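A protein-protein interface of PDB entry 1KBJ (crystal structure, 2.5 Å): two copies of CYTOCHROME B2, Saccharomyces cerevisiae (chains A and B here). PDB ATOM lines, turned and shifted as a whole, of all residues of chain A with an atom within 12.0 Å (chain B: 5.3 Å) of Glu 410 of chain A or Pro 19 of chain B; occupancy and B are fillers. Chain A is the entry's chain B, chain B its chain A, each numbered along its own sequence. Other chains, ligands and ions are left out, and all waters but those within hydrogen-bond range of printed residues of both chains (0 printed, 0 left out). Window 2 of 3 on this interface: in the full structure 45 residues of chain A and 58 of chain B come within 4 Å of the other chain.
Among the printed residues, pairs that only touch across the chains: Glu 408 of chain A with Pro 18 of chain B (3.7 Å), Phe 409 of chain A with Leu 16 of chain B (3.4 Å), Phe 409 of chain A with Leu 17 of chain B (3.3 Å), Glu 410 of chain A with Leu 17 of chain B (3.9 Å), Glu 410 of chain A with Pro 18 of chain B (3.5 Å) and Glu 410 of chain A with Pro 19 of chain B (3.0 Å).
No position is printed for both chains. Of the 7 pairs that touch across the chains among the printed residues, none has its exchanged pair printed and touching as well.
Of the 7 printed residues of chain A, 3 touch a printed residue of chain B. Hydrophobic or aromatic side chains of chain A within 4 Å of the printed part of chain B: Phe 409. Of the 9 printed residues of chain B, 4 touch a printed residue of chain A. Printed residues of chain B that touch a printed residue of chain A: Leu 16, Leu 17, Pro 18 and Pro 19. Among the printed residues, 7 pairs touch across the chains. Among the printed residues, no Asp or Glu carboxylate lies within 4 Å of a Lys or Arg side-chain nitrogen of the other chain.
The backbone carbonyl oxygen of Leu 16 of chain B is in hydrogen-bond range of the backbone NH of Glu 410 of chain A.
The backbone carbonyl oxygen of Pro 18 of chain B is in hydrogen-bond range of the side-chain hydroxyl of Tyr 343 of chain B, 2.6 Å away.
Of chain B, only Leu 16, Leu 17, Pro 18 and Pro 19 come within 4 Å of Glu 410 of chain A. Of chain A, only Glu 410 comes within 4 Å of Pro 19 of chain B. Pro 18 of chain B touches just these residues of chain A: Glu 408 (3.7 Å) and Glu 410 (3.5 Å). No residue of chain A comes within 4 Å of Leu 20 of chain B. No residue of chain A comes within 4 Å of Asp 21 of chain B. No residue of chain A comes within 4 Å of Asn 22 of chain B. Of the printed residues of chain A, Leu 17 of chain B touches Phe 409 and Glu 410. Of the printed residues of chain B, Glu 408 of chain A touches Pro 18. Of the printed residues of chain B, Phe 409 of chain A touches Leu 16 and Leu 17. The nearest residue of chain A that does not touch Pro 19 of chain B is Thr 407 of chain A (6.7 Å).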
ATOM      1  N   LEU A 406      31.709 -14.235  15.475  1.00  0.00           N
ATOM      2  CA  LEU A 406      30.500 -14.646  14.796  1.00  0.00           C
ATOM      3  C   LEU A 406      29.587 -15.327  15.807  1.00  0.00           C
ATOM      4  O   LEU A 406      30.050 -15.844  16.831  1.00  0.00           O
ATOM      5  CB  LEU A 406      30.871 -15.606  13.666  1.00  0.00           C
ATOM      6  CG  LEU A 406      31.579 -14.890  12.508  1.00  0.00           C
ATOM      7  CD1 LEU A 406      32.504 -15.838  11.732  1.00  0.00           C
ATOM      8  CD2 LEU A 406      30.500 -14.289  11.613  1.00  0.00           C
ATOM      9  N   THR A 407      28.291 -15.308  15.530  1.00  0.00           N
ATOM     10  CA  THR A 407      27.328 -15.950  16.402  1.00  0.00           C
ATOM     11  C   THR A 407      27.701 -17.437  16.474  1.00  0.00           C
ATOM     12  O   THR A 407      28.421 -17.941  15.617  1.00  0.00           O
ATOM     13  CB  THR A 407      25.954 -15.854  15.810  1.00  0.00           C
ATOM     14  OG1 THR A 407      24.989 -16.285  16.777  1.00  0.00           O
ATOM     15  CG2 THR A 407      25.884 -16.727  14.564  1.00  0.00           C
ATOM     16  N   GLU A 408      27.202 -18.152  17.473  1.00  0.00           N
ATOM     17  CA  GLU A 408      27.542 -19.563  17.597  1.00  0.00           C
ATOM     18  C   GLU A 408      26.327 -20.468  17.627  1.00  0.00           C
ATOM     19  O   GLU A 408      25.210 -20.021  17.936  1.00  0.00           O
ATOM     20  CB  GLU A 408      28.322 -19.791  18.873  1.00  0.00           C
ATOM     21  CG  GLU A 408      29.248 -18.652  19.246  1.00  0.00           C
ATOM     22  CD  GLU A 408      30.060 -18.965  20.499  1.00  0.00           C
ATOM     23  OE1 GLU A 408      31.023 -19.762  20.400  1.00  0.00           O
ATOM     24  OE2 GLU A 408      29.727 -18.433  21.587  1.00  0.00           O
ATOM     25  N   PHE A 409      26.545 -21.742  17.306  1.00  0.00           N
ATOM     26  CA  PHE A 409      25.463 -22.715  17.357  1.00  0.00           C
ATOM     27  C   PHE A 409      25.077 -22.932  18.814  1.00  0.00           C
ATOM     28  O   PHE A 409      25.875 -22.674  19.702  1.00  0.00           O
ATOM     29  CB  PHE A 409      25.902 -24.031  16.731  1.00  0.00           C
ATOM     30  CG  PHE A 409      25.935 -23.992  15.237  1.00  0.00           C
ATOM     31  CD1 PHE A 409      27.111 -23.701  14.567  1.00  0.00           C
ATOM     32  CD2 PHE A 409      24.768 -24.197  14.498  1.00  0.00           C
ATOM     33  CE1 PHE A 409      27.139 -23.612  13.186  1.00  0.00           C
ATOM     34  CE2 PHE A 409      24.778 -24.112  13.112  1.00  0.00           C
ATOM     35  CZ  PHE A 409      25.967 -23.818  12.445  1.00  0.00           C
ATOM     36  N   GLU A 410      23.850 -23.381  19.062  1.00  0.00           N
ATOM     37  CA  GLU A 410      23.405 -23.625  20.425  1.00  0.00           C
ATOM     38  C   GLU A 410      24.289 -24.701  21.034  1.00  0.00           C
ATOM     39  O   GLU A 410      24.894 -25.487  20.318  1.00  0.00           O
ATOM     40  CB  GLU A 410      21.948 -24.107  20.441  1.00  0.00           C
ATOM     41  CG  GLU A 410      20.896 -23.023  20.330  1.00  0.00           C
ATOM     42  CD  GLU A 410      21.209 -21.834  21.212  1.00  0.00           C
ATOM     43  OE1 GLU A 410      21.818 -22.014  22.294  1.00  0.00           O
ATOM     44  OE2 GLU A 410      20.840 -20.711  20.822  1.00  0.00           O
ATOM     45  N   ASP A 411      24.378 -24.736  22.355  1.00  0.00           N
ATOM     46  CA  ASP A 411      25.174 -25.768  23.011  1.00  0.00           C
ATOM     47  C   ASP A 411      24.494 -27.113  22.847  1.00  0.00           C
ATOM     48  O   ASP A 411      23.351 -27.292  23.276  1.00  0.00           O
ATOM     49  CB  ASP A 411      25.340 -25.468  24.496  1.00  0.00           C
ATOM     50  CG  ASP A 411      26.462 -24.496  24.758  1.00  0.00           C
ATOM     51  OD1 ASP A 411      27.482 -24.603  24.045  1.00  0.00           O
ATOM     52  OD2 ASP A 411      26.339 -23.645  25.668  1.00  0.00           O
ATOM     53  N   ALA A 412      25.208 -28.042  22.219  1.00  0.00           N
ATOM     54  CA  ALA A 412      24.702 -29.381  21.968  1.00  0.00           C
ATOM     55  C   ALA A 412      23.966 -29.910  23.203  1.00  0.00           C
ATOM     56  O   ALA A 412      22.774 -30.311  23.078  1.00  0.00           O
ATOM     57  CB  ALA A 412      25.862 -30.309  21.592  1.00  0.00           C
ATOM     58  OXT ALA A 412      24.604 -29.901  24.285  1.00  0.00           O
ATOM     59  N   LEU B  16      20.839 -27.143  16.243  1.00  0.00           N
ATOM     60  CA  LEU B  16      21.462 -26.264  17.211  1.00  0.00           C
ATOM     61  C   LEU B  16      21.527 -24.846  16.672  1.00  0.00           C
ATOM     62  O   LEU B  16      22.191 -23.987  17.248  1.00  0.00           O
ATOM     63  CB  LEU B  16      22.871 -26.740  17.547  1.00  0.00           C
ATOM     64  CG  LEU B  16      23.083 -27.854  18.579  1.00  0.00           C
ATOM     65  CD1 LEU B  16      21.839 -28.076  19.416  1.00  0.00           C
ATOM     66  CD2 LEU B  16      23.469 -29.102  17.864  1.00  0.00           C
ATOM     67  N   LEU B  17      20.867 -24.604  15.545  1.00  0.00           N
ATOM     68  CA  LEU B  17      20.842 -23.263  14.962  1.00  0.00           C
ATOM     69  C   LEU B  17      20.337 -22.330  16.082  1.00  0.00           C
ATOM     70  O   LEU B  17      19.372 -22.647  16.769  1.00  0.00           O
ATOM     71  CB  LEU B  17      19.876 -23.254  13.782  1.00  0.00           C
ATOM     72  CG  LEU B  17      20.315 -22.885  12.372  1.00  0.00           C
ATOM     73  CD1 LEU B  17      21.805 -22.944  12.227  1.00  0.00           C
ATOM     74  CD2 LEU B  17      19.649 -23.842  11.396  1.00  0.00           C
ATOM     75  N   PRO B  18      20.992 -21.181  16.297  1.00  0.00           N
ATOM     76  CA  PRO B  18      20.508 -20.295  17.367  1.00  0.00           C
ATOM     77  C   PRO B  18      19.183 -19.609  17.011  1.00  0.00           C
ATOM     78  O   PRO B  18      18.788 -19.568  15.846  1.00  0.00           O
ATOM     79  CB  PRO B  18      21.651 -19.304  17.525  1.00  0.00           C
ATOM     80  CG  PRO B  18      22.165 -19.157  16.104  1.00  0.00           C
ATOM     81  CD  PRO B  18      22.126 -20.581  15.560  1.00  0.00           C
ATOM     82  N   PRO B  19      18.469 -19.077  18.011  1.00  0.00           N
ATOM     83  CA  PRO B  19      17.209 -18.419  17.670  1.00  0.00           C
ATOM     84  C   PRO B  19      17.396 -17.238  16.729  1.00  0.00           C
ATOM     85  O   PRO B  19      18.242 -16.349  16.940  1.00  0.00           O
ATOM     86  CB  PRO B  19      16.636 -18.011  19.032  1.00  0.00           C
ATOM     87  CG  PRO B  19      17.821 -18.015  19.944  1.00  0.00           C
ATOM     88  CD  PRO B  19      18.626 -19.178  19.472  1.00  0.00           C
ATOM     89  N   LEU B  20      16.579 -17.232  15.688  1.00  0.00           N
ATOM     90  CA  LEU B  20      16.625 -16.195  14.687  1.00  0.00           C
ATOM     91  C   LEU B  20      16.870 -14.782  15.216  1.00  0.00           C
ATOM     92  O   LEU B  20      17.598 -14.036  14.585  1.00  0.00           O
ATOM     93  CB  LEU B  20      15.349 -16.238  13.845  1.00  0.00           C
ATOM     94  CG  LEU B  20      15.388 -15.443  12.541  1.00  0.00           C
ATOM     95  CD1 LEU B  20      16.673 -15.803  11.759  1.00  0.00           C
ATOM     96  CD2 LEU B  20      14.122 -15.743  11.718  1.00  0.00           C
ATOM     97  N   ASP B  21      16.313 -14.385  16.355  1.00  0.00           N
ATOM     98  CA  ASP B  21      16.592 -13.015  16.760  1.00  0.00           C
ATOM     99  C   ASP B  21      17.853 -12.832  17.584  1.00  0.00           C
ATOM    100  O   ASP B  21      18.052 -11.805  18.247  1.00  0.00           O
ATOM    101  CB  ASP B  21      15.386 -12.352  17.439  1.00  0.00           C
ATOM    102  CG  ASP B  21      14.649 -13.282  18.346  1.00  0.00           C
ATOM    103  OD1 ASP B  21      15.281 -13.802  19.301  1.00  0.00           O
ATOM    104  OD2 ASP B  21      13.433 -13.490  18.094  1.00  0.00           O
ATOM    105  N   ASN B  22      18.723 -13.829  17.522  1.00  0.00           N
ATOM    106  CA  ASN B  22      20.008 -13.737  18.206  1.00  0.00           C
ATOM    107  C   ASN B  22      21.038 -13.428  17.103  1.00  0.00           C
ATOM    108  O   ASN B  22      22.228 -13.216  17.378  1.00  0.00           O
ATOM    109  CB  ASN B  22      20.357 -15.061  18.901  1.00  0.00           C
ATOM    110  CG  ASN B  22      19.756 -15.173  20.300  1.00  0.00           C
ATOM    111  OD1 ASN B  22      18.680 -14.623  20.579  1.00  0.00           O
ATOM    112  ND2 ASN B  22      20.447 -15.902  21.183  1.00  0.00           N
ATOM    113  N   ILE B  23      20.555 -13.432  15.856  1.00  0.00           N
ATOM    114  CA  ILE B  23      21.361 -13.123  14.671  1.00  0.00           C
ATOM    115  C   ILE B  23      21.552 -11.596  14.677  1.00  0.00           C
ATOM    116  O   ILE B  23      20.577 -10.846  14.581  1.00  0.00           O
ATOM    117  CB  ILE B  23      20.627 -13.550  13.372  1.00  0.00           C
ATOM    118  CG1 ILE B  23      20.345 -15.053  13.417  1.00  0.00           C
ATOM    119  CG2 ILE B  23      21.447 -13.162  12.139  1.00  0.00           C
ATOM    120  CD1 ILE B  23      21.586 -15.911  13.489  1.00  0.00           C
ATOM    121  N   TYR B 343      17.377 -20.208   7.572  1.00  0.00           N
ATOM    122  CA  TYR B 343      16.152 -19.908   8.294  1.00  0.00           C
ATOM    123  C   TYR B 343      14.938 -19.720   7.410  1.00  0.00           C
ATOM    124  O   TYR B 343      13.867 -19.393   7.910  1.00  0.00           O
ATOM    125  CB  TYR B 343      16.346 -18.658   9.147  1.00  0.00           C
ATOM    126  CG  TYR B 343      17.299 -18.852  10.300  1.00  0.00           C
ATOM    127  CD1 TYR B 343      16.849 -19.324  11.529  1.00  0.00           C
ATOM    128  CD2 TYR B 343      18.650 -18.528  10.173  1.00  0.00           C
ATOM    129  CE1 TYR B 343      17.726 -19.459  12.613  1.00  0.00           C
ATOM    130  CE2 TYR B 343      19.531 -18.665  11.244  1.00  0.00           C
ATOM    131  CZ  TYR B 343      19.067 -19.128  12.458  1.00  0.00           C
ATOM    132  OH  TYR B 343      19.953 -19.250  13.505  1.00  0.00           O
